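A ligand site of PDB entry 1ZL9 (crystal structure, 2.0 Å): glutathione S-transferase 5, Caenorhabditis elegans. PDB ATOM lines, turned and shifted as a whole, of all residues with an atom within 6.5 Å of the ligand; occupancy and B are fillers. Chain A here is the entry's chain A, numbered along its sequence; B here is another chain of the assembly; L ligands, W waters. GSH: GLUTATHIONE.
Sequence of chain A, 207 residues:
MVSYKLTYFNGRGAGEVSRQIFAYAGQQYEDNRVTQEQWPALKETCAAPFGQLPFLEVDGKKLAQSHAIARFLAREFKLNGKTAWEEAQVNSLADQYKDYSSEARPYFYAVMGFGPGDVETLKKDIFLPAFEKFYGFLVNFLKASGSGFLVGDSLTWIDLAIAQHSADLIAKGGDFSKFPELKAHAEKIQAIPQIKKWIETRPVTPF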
ATOM      1  N   TYR A   8      11.002  25.451  12.931  1.00  0.00           N
ATOM      2  CA  TYR A   8      10.474  24.468  12.000  1.00  0.00           C
ATOM      3  C   TYR A   8      11.322  23.195  12.136  1.00  0.00           C
ATOM      4  O   TYR A   8      12.231  23.181  12.919  1.00  0.00           O
ATOM      5  CB  TYR A   8      10.476  25.039  10.566  1.00  0.00           C
ATOM      6  CG  TYR A   8       9.770  24.206   9.526  1.00  0.00           C
ATOM      7  CD1 TYR A   8       8.440  23.916   9.636  1.00  0.00           C
ATOM      8  CD2 TYR A   8      10.467  23.639   8.408  1.00  0.00           C
ATOM      9  CE1 TYR A   8       7.795  23.149   8.677  1.00  0.00           C
ATOM     10  CE2 TYR A   8       9.825  22.851   7.490  1.00  0.00           C
ATOM     11  CZ  TYR A   8       8.496  22.611   7.611  1.00  0.00           C
ATOM     12  OH  TYR A   8       7.840  21.824   6.650  1.00  0.00           O
ATOM     13  N   PHE A   9      10.947  22.141  11.431  1.00  0.00           N
ATOM     14  CA  PHE A   9      11.755  20.914  11.329  1.00  0.00           C
ATOM     15  C   PHE A   9      13.066  21.134  10.547  1.00  0.00           C
ATOM     16  O   PHE A   9      13.280  22.194   9.910  1.00  0.00           O
ATOM     17  CB  PHE A   9      10.913  19.800  10.731  1.00  0.00           C
ATOM     18  CG  PHE A   9       9.730  19.483  11.573  1.00  0.00           C
ATOM     19  CD1 PHE A   9       9.917  18.915  12.834  1.00  0.00           C
ATOM     20  CD2 PHE A   9       8.444  19.829  11.158  1.00  0.00           C
ATOM     21  CE1 PHE A   9       8.799  18.655  13.667  1.00  0.00           C
ATOM     22  CE2 PHE A   9       7.358  19.587  11.986  1.00  0.00           C
ATOM     23  CZ  PHE A   9       7.510  19.002  13.211  1.00  0.00           C
ATOM     24  N   ALA A  14       7.880  23.765   4.513  1.00  0.00           N
ATOM     25  CA  ALA A  14       7.054  24.974   4.592  1.00  0.00           C
ATOM     26  C   ALA A  14       7.785  26.172   5.274  1.00  0.00           C
ATOM     27  O   ALA A  14       7.330  27.306   5.169  1.00  0.00           O
ATOM     28  CB  ALA A  14       5.783  24.622   5.339  1.00  0.00           C
ATOM     29  N   TRP A  39      10.256  17.460  19.623  1.00  0.00           N
ATOM     30  CA  TRP A  39       8.948  17.870  19.052  1.00  0.00           C
ATOM     31  C   TRP A  39       7.737  17.552  20.001  1.00  0.00           C
ATOM     32  O   TRP A  39       7.152  18.502  20.593  1.00  0.00           O
ATOM     33  CB  TRP A  39       8.756  17.380  17.560  1.00  0.00           C
ATOM     34  CG  TRP A  39       7.366  17.693  17.027  1.00  0.00           C
ATOM     35  CD1 TRP A  39       6.460  16.822  16.461  1.00  0.00           C
ATOM     36  CD2 TRP A  39       6.728  18.943  17.086  1.00  0.00           C
ATOM     37  NE1 TRP A  39       5.289  17.481  16.188  1.00  0.00           N
ATOM     38  CE2 TRP A  39       5.423  18.781  16.573  1.00  0.00           C
ATOM     39  CE3 TRP A  39       7.099  20.190  17.559  1.00  0.00           C
ATOM     40  CZ2 TRP A  39       4.519  19.815  16.517  1.00  0.00           C
ATOM     41  CZ3 TRP A  39       6.197  21.215  17.493  1.00  0.00           C
ATOM     42  CH2 TRP A  39       4.926  21.021  16.944  1.00  0.00           C
ATOM     43  N   LYS A  43       5.381  20.205  21.416  1.00  0.00           N
ATOM     44  CA  LYS A  43       3.976  20.115  21.111  1.00  0.00           C
ATOM     45  C   LYS A  43       3.105  20.097  22.369  1.00  0.00           C
ATOM     46  O   LYS A  43       2.108  20.864  22.438  1.00  0.00           O
ATOM     47  CB  LYS A  43       3.676  18.900  20.265  1.00  0.00           C
ATOM     48  CG  LYS A  43       2.324  19.022  19.624  1.00  0.00           C
ATOM     49  CD  LYS A  43       1.871  17.761  18.956  1.00  0.00           C
ATOM     50  CE  LYS A  43       0.468  17.925  18.399  1.00  0.00           C
ATOM     51  NZ  LYS A  43       0.463  18.026  16.931  1.00  0.00           N
ATOM     52  N   PHE A  50      -1.196  26.675  16.828  1.00  0.00           N
ATOM     53  CA  PHE A  50      -2.091  25.622  16.394  1.00  0.00           C
ATOM     54  C   PHE A  50      -1.494  24.251  16.490  1.00  0.00           C
ATOM     55  O   PHE A  50      -1.921  23.330  15.767  1.00  0.00           O
ATOM     56  CB  PHE A  50      -2.582  25.875  14.971  1.00  0.00           C
ATOM     57  CG  PHE A  50      -3.124  27.245  14.782  1.00  0.00           C
ATOM     58  CD1 PHE A  50      -2.626  28.057  13.753  1.00  0.00           C
ATOM     59  CD2 PHE A  50      -4.095  27.758  15.634  1.00  0.00           C
ATOM     60  CE1 PHE A  50      -3.127  29.325  13.530  1.00  0.00           C
ATOM     61  CE2 PHE A  50      -4.625  29.078  15.416  1.00  0.00           C
ATOM     62  CZ  PHE A  50      -4.109  29.869  14.390  1.00  0.00           C
ATOM     63  N   GLY A  51      -0.525  24.093  17.362  1.00  0.00           N
ATOM     64  CA  GLY A  51       0.063  22.771  17.589  1.00  0.00           C
ATOM     65  C   GLY A  51       0.969  22.284  16.464  1.00  0.00           C
ATOM     66  O   GLY A  51       1.286  21.079  16.395  1.00  0.00           O
ATOM     67  N   GLN A  52       1.312  23.163  15.532  1.00  0.00           N
ATOM     68  CA  GLN A  52       2.057  22.704  14.342  1.00  0.00           C
ATOM     69  C   GLN A  52       3.185  23.698  13.992  1.00  0.00           C
ATOM     70  O   GLN A  52       3.143  24.834  14.479  1.00  0.00           O
ATOM     71  CB  GLN A  52       1.117  22.545  13.127  1.00  0.00           C
ATOM     72  CG  GLN A  52       0.122  21.387  13.356  1.00  0.00           C
ATOM     73  CD  GLN A  52      -0.534  20.935  12.114  1.00  0.00           C
ATOM     74  OE1 GLN A  52      -0.337  19.791  11.671  1.00  0.00           O
ATOM     75  NE2 GLN A  52      -1.319  21.821  11.519  1.00  0.00           N
ATOM     76  N   LEU A  53       4.148  23.265  13.160  1.00  0.00           N
ATOM     77  CA  LEU A  53       5.222  24.123  12.659  1.00  0.00           C
ATOM     78  C   LEU A  53       4.955  24.387  11.170  1.00  0.00           C
ATOM     79  O   LEU A  53       4.291  23.586  10.511  1.00  0.00           O
ATOM     80  CB  LEU A  53       6.592  23.406  12.811  1.00  0.00           C
ATOM     81  CG  LEU A  53       6.912  22.860  14.205  1.00  0.00           C
ATOM     82  CD1 LEU A  53       8.367  22.280  14.312  1.00  0.00           C
ATOM     83  CD2 LEU A  53       6.645  24.000  15.214  1.00  0.00           C
ATOM     84  N   PRO A  54       5.461  25.472  10.620  1.00  0.00           N
ATOM     85  CA  PRO A  54       6.287  26.465  11.336  1.00  0.00           C
ATOM     86  C   PRO A  54       5.551  27.478  12.198  1.00  0.00           C
ATOM     87  O   PRO A  54       4.330  27.647  12.085  1.00  0.00           O
ATOM     88  CB  PRO A  54       6.946  27.232  10.170  1.00  0.00           C
ATOM     89  CG  PRO A  54       5.890  27.196   9.090  1.00  0.00           C
ATOM     90  CD  PRO A  54       5.269  25.862   9.205  1.00  0.00           C
ATOM     91  N   ALA A  64       1.844  31.725  13.671  1.00  0.00           N
ATOM     92  CA  ALA A  64       1.772  30.456  12.973  1.00  0.00           C
ATOM     93  C   ALA A  64       1.289  30.630  11.540  1.00  0.00           C
ATOM     94  O   ALA A  64       0.816  31.709  11.148  1.00  0.00           O
ATOM     95  CB  ALA A  64       0.774  29.622  13.699  1.00  0.00           C
ATOM     96  N   GLN A  65       1.328  29.507  10.819  1.00  0.00           N
ATOM     97  CA  GLN A  65       0.850  29.329   9.435  1.00  0.00           C
ATOM     98  C   GLN A  65       1.845  29.828   8.372  1.00  0.00           C
ATOM     99  O   GLN A  65       2.120  31.018   8.283  1.00  0.00           O
ATOM    100  CB  GLN A  65      -0.539  29.927   9.238  1.00  0.00           C
ATOM    101  CG  GLN A  65      -1.631  28.997   9.888  1.00  0.00           C
ATOM    102  CD  GLN A  65      -2.024  27.796   9.058  1.00  0.00           C
ATOM    103  OE1 GLN A  65      -2.781  26.904   9.528  1.00  0.00           O
ATOM    104  NE2 GLN A  65      -1.571  27.752   7.854  1.00  0.00           N
ATOM    105  N   SER A  66       2.405  28.882   7.615  1.00  0.00           N
ATOM    106  CA  SER A  66       3.487  29.145   6.695  1.00  0.00           C
ATOM    107  C   SER A  66       3.274  30.339   5.788  1.00  0.00           C
ATOM    108  O   SER A  66       4.225  31.128   5.662  1.00  0.00           O
ATOM    109  CB  SER A  66       3.821  27.890   5.869  1.00  0.00           C
ATOM    110  OG  SER A  66       2.779  27.490   5.032  1.00  0.00           O
ATOM    111  N   HIS A  67       2.066  30.474   5.202  1.00  0.00           N
ATOM    112  CA  HIS A  67       1.746  31.563   4.298  1.00  0.00           C
ATOM    113  C   HIS A  67       1.595  32.881   5.083  1.00  0.00           C
ATOM    114  O   HIS A  67       2.000  33.920   4.577  1.00  0.00           O
ATOM    115  CB  HIS A  67       0.495  31.344   3.428  1.00  0.00           C
ATOM    116  CG  HIS A  67       0.667  30.371   2.305  1.00  0.00           C
ATOM    117  ND1 HIS A  67       1.151  30.706   1.088  1.00  0.00           N
ATOM    118  CD2 HIS A  67       0.216  29.113   2.143  1.00  0.00           C
ATOM    119  CE1 HIS A  67       1.206  29.654   0.289  1.00  0.00           C
ATOM    120  NE2 HIS A  67       0.653  28.659   0.913  1.00  0.00           N
ATOM    121  N   ILE A  69       3.158  33.719   7.879  1.00  0.00           N
ATOM    122  CA  ILE A  69       4.495  34.113   8.136  1.00  0.00           C
ATOM    123  C   ILE A  69       5.193  34.709   6.925  1.00  0.00           C
ATOM    124  O   ILE A  69       5.775  35.771   7.035  1.00  0.00           O
ATOM    125  CB  ILE A  69       5.261  32.918   8.685  1.00  0.00           C
ATOM    126  CG1 ILE A  69       4.660  32.447  10.024  1.00  0.00           C
ATOM    127  CG2 ILE A  69       6.712  33.228   8.898  1.00  0.00           C
ATOM    128  CD1 ILE A  69       5.064  31.050  10.433  1.00  0.00           C
ATOM    129  N   LYS A  98      -1.262  26.416  -2.587  1.00  0.00           N
ATOM    130  CA  LYS A  98      -1.826  25.586  -1.528  1.00  0.00           C
ATOM    131  C   LYS A  98      -2.781  24.537  -2.032  1.00  0.00           C
ATOM    132  O   LYS A  98      -2.753  23.427  -1.529  1.00  0.00           O
ATOM    133  CB  LYS A  98      -2.626  26.410  -0.516  1.00  0.00           C
ATOM    134  CG  LYS A  98      -2.030  26.714   0.736  1.00  0.00           C
ATOM    135  CD  LYS A  98      -3.129  27.121   1.778  1.00  0.00           C
ATOM    136  CE  LYS A  98      -2.567  28.051   2.867  1.00  0.00           C
ATOM    137  NZ  LYS A  98      -1.737  27.337   3.865  1.00  0.00           N
ATOM    138  N   TYR A 109       3.486  12.654   0.485  1.00  0.00           N
ATOM    139  CA  TYR A 109       3.506  11.865   1.708  1.00  0.00           C
ATOM    140  C   TYR A 109       4.020  10.452   1.547  1.00  0.00           C
ATOM    141  O   TYR A 109       4.690   9.917   2.460  1.00  0.00           O
ATOM    142  CB  TYR A 109       2.114  11.811   2.286  1.00  0.00           C
ATOM    143  CG  TYR A 109       1.905  12.858   3.282  1.00  0.00           C
ATOM    144  CD1 TYR A 109       2.270  14.156   3.046  1.00  0.00           C
ATOM    145  CD2 TYR A 109       1.273  12.550   4.486  1.00  0.00           C
ATOM    146  CE1 TYR A 109       2.055  15.154   4.001  1.00  0.00           C
ATOM    147  CE2 TYR A 109       1.058  13.538   5.441  1.00  0.00           C
ATOM    148  CZ  TYR A 109       1.463  14.814   5.200  1.00  0.00           C
ATOM    149  OH  TYR A 109       1.246  15.761   6.154  1.00  0.00           O
ATOM    150  N   PHE A 114       5.454   9.075   4.916  1.00  0.00           N
ATOM    151  CA  PHE A 114       4.396   9.371   5.863  1.00  0.00           C
ATOM    152  C   PHE A 114       3.079   8.757   5.477  1.00  0.00           C
ATOM    153  O   PHE A 114       2.194   8.647   6.287  1.00  0.00           O
ATOM    154  CB  PHE A 114       4.156  10.882   5.987  1.00  0.00           C
ATOM    155  CG  PHE A 114       5.366  11.660   6.459  1.00  0.00           C
ATOM    156  CD1 PHE A 114       6.311  11.083   7.284  1.00  0.00           C
ATOM    157  CD2 PHE A 114       5.531  12.969   6.079  1.00  0.00           C
ATOM    158  CE1 PHE A 114       7.439  11.835   7.753  1.00  0.00           C
ATOM    159  CE2 PHE A 114       6.655  13.712   6.506  1.00  0.00           C
ATOM    160  CZ  PHE A 114       7.599  13.145   7.342  1.00  0.00           C
ATOM    161  N   ASP B  95      -6.029  31.007   7.631  1.00  0.00           N
ATOM    162  CA  ASP B  95      -5.409  29.825   7.064  1.00  0.00           C
ATOM    163  C   ASP B  95      -5.683  28.594   7.903  1.00  0.00           C
ATOM    164  O   ASP B  95      -5.822  27.507   7.357  1.00  0.00           O
ATOM    165  CB  ASP B  95      -3.865  30.066   6.866  1.00  0.00           C
ATOM    166  CG  ASP B  95      -3.558  30.920   5.645  1.00  0.00           C
ATOM    167  OD1 ASP B  95      -4.554  31.447   4.994  1.00  0.00           O
ATOM    168  OD2 ASP B  95      -2.376  31.062   5.206  1.00  0.00           O
ATOM    169  N   GLN B  96      -5.767  28.749   9.237  1.00  0.00           N
ATOM    170  CA  GLN B  96      -6.117  27.632  10.075  1.00  0.00           C
ATOM    171  C   GLN B  96      -7.602  27.235   9.795  1.00  0.00           C
ATOM    172  O   GLN B  96      -7.923  26.068   9.796  1.00  0.00           O
ATOM    173  CB  GLN B  96      -5.902  27.941  11.559  1.00  0.00           C
ATOM    174  CG  GLN B  96      -6.117  26.707  12.469  1.00  0.00           C
ATOM    175  CD  GLN B  96      -5.149  25.594  12.220  1.00  0.00           C
ATOM    176  OE1 GLN B  96      -3.986  25.845  11.871  1.00  0.00           O
ATOM    177  NE2 GLN B  96      -5.600  24.320  12.433  1.00  0.00           N
ATOM    178  N   ASP B  99      -7.647  24.955   6.957  1.00  0.00           N
ATOM    179  CA  ASP B  99      -7.246  23.589   7.325  1.00  0.00           C
ATOM    180  C   ASP B  99      -8.445  22.845   8.010  1.00  0.00           C
ATOM    181  O   ASP B  99      -8.660  21.626   7.775  1.00  0.00           O
ATOM    182  CB  ASP B  99      -6.020  23.598   8.290  1.00  0.00           C
ATOM    183  CG  ASP B  99      -4.713  24.058   7.611  1.00  0.00           C
ATOM    184  OD1 ASP B  99      -4.611  24.101   6.341  1.00  0.00           O
ATOM    185  OD2 ASP B  99      -3.702  24.351   8.290  1.00  0.00           O
HETATM  186  N1  GSH L   1      -1.489  25.095   7.160  1.00  0.00           N
HETATM  187  CA1 GSH L   1      -0.207  24.718   7.655  1.00  0.00           C
HETATM  188  C1  GSH L   1       0.845  25.695   7.334  1.00  0.00           C
HETATM  189  O11 GSH L   1       1.768  26.110   8.223  1.00  0.00           O
HETATM  190  O12 GSH L   1       0.937  26.079   6.105  1.00  0.00           O
HETATM  191  CB1 GSH L   1       0.142  23.315   8.025  1.00  0.00           C
HETATM  192  CG1 GSH L   1       1.181  23.150   9.152  1.00  0.00           C
HETATM  193  CD1 GSH L   1       1.591  21.698   9.248  1.00  0.00           C
HETATM  194  OE1 GSH L   1       0.820  20.782   8.592  1.00  0.00           O
HETATM  195  N2  GSH L   1       2.631  21.318   9.988  1.00  0.00           N
HETATM  196  CA2 GSH L   1       3.135  19.983   9.978  1.00  0.00           C
HETATM  197  C2  GSH L   1       3.323  19.574  11.413  1.00  0.00           C
HETATM  198  O2  GSH L   1       3.807  20.550  12.236  1.00  0.00           O
HETATM  199  CB2 GSH L   1       4.448  20.103   9.216  1.00  0.00           C
HETATM  200  SG2 GSH L   1       5.268  18.494   9.174  1.00  0.00           S
HETATM  201  N3  GSH L   1       3.104  18.346  11.835  1.00  0.00           N
HETATM  202  CA3 GSH L   1       3.456  17.850  13.164  1.00  0.00           C
HETATM  203  C3  GSH L   1       2.227  17.745  14.041  1.00  0.00           C
HETATM  204  O31 GSH L   1       0.992  18.130  13.512  1.00  0.00           O
HETATM  205  O32 GSH L   1       2.273  17.354  15.291  1.00  0.00           O
HETATM  206  O   HOH W   1      -0.447  29.163   5.683  1.00  0.00           O
HETATM  207  O   HOH W   2       5.052  21.264   6.607  1.00  0.00           O
HETATM  208  O   HOH W   3       3.137  23.583   6.803  1.00  0.00           O
HETATM  209  O   HOH W   4      -1.287  18.207  14.861  1.00  0.00           O
HETATM  210  O   HOH W   5       2.161  26.635  10.821  1.00  0.00           O
HETATM  211  O   HOH W   6       1.093  16.883  10.138  1.00  0.00           O
HETATM  212  O   HOH W   7      -2.209  20.389   7.438  1.00  0.00           O
HETATM  213  O   HOH W   8      -3.734  26.566   5.475  1.00  0.00           O
HETATM  214  O   HOH W   9       1.778  18.591   6.097  1.00  0.00           O
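The backbone carbonyl oxygen (O) of Leu 53 sits at hydrogen-bond distance from a nitrogen (N2) of the ligand.
The side-chain hydroxyl (OG) of Ser 66 is in hydrogen-bond range of an oxygen (O12) of the ligand.
The indole nitrogen (NE1) of Trp 39 sits at hydrogen-bond distance from an oxygen (O32) of the ligand.
N1 of the ligand lies within salt-bridge range of OD2 of Asp 99 of chain B, at 2.6 Å.
The backbone NH (N) of Leu 53 sits at hydrogen-bond distance from an oxygen (O2) of the ligand, at 2.9 Å.
The side-chain amino group (NZ) of Lys 43 lies within salt-bridge range of an oxygen (O32) of the ligand, at 2.5 Å.
An oxygen (O12) of the ligand lies within salt-bridge range of the side-chain amino group (NZ) of Lys 98 (3.7 Å).
N of Ser 66 is in hydrogen-bond range of O11 of the ligand (2.9 Å).
NE2 of Gln 65 sits close to N1 of the ligand (2.7 Å).
An oxygen (O31) of the ligand lies close to the side-chain amide oxygen (OE1) of Gln 52, 2.8 Å away.
The side-chain amide oxygen (OE1) of Gln 96 of chain B sits close to the side-chain amide oxygen (OE1) of Gln 65, at 2.8 Å.
The side-chain amide oxygen of Gln 65 sits close to the side-chain carboxylate of Asp 99 of chain B (3.0 Å).
O of Gly 51 sits at hydrogen-bond distance from NZ of Lys 43.
Phe 9 touches the ligand (CE2 to SG2, 3.7 Å).
Pro 54 touches the ligand (CD to O11, 3.6 Å).
Hydrophobic or aromatic side chains that line the ligand: Phe 9, Trp 39 and Pro 54.
Ten residues have an atom within 4 Å of the ligand: Phe 9, Trp 39, Lys 43, Gln 52, Leu 53, Pro 54, Gln 65, Ser 66, Lys 98 and Asp 99 of chain B.
The nearest printed residue that does not touch the ligand is Gly 51 (4.01 Å).
Water W4 bridges an oxygen (O31) of the ligand (2.6 Å) and the side-chain amino group (NZ) of Lys 43 (2.7 Å).
Water W5 lies within hydrogen-bond range of an oxygen (O11) of the ligand (2.7 Å), the backbone carbonyl oxygen of Pro 54 (2.7 Å) and the backbone NH of Gln 65 (3.0 Å).
Water W2 bridges the side-chain hydroxyl (OH) of Tyr 8 (2.8 Å) and a sulfur (SG2) of the ligand (3.8 Å).
Water W8 lies within hydrogen-bond range of the side-chain amino group (NZ) of Lys 98 (2.7 Å), the side-chain carboxylate (OD1) of Asp 99 of chain B (2.8 Å), the backbone carbonyl oxygen (O) of Asp 95 of chain B (3.0 Å), a nitrogen (N1) of the ligand (3.2 Å) and the side-chain amide nitrogen (NE2) of Gln 65 (3.4 Å).
Water W9 lies within hydrogen-bond range of the side-chain hydroxyl of Tyr 109 (2.9 Å) and an oxygen (OE1) of the ligand (3.5 Å).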
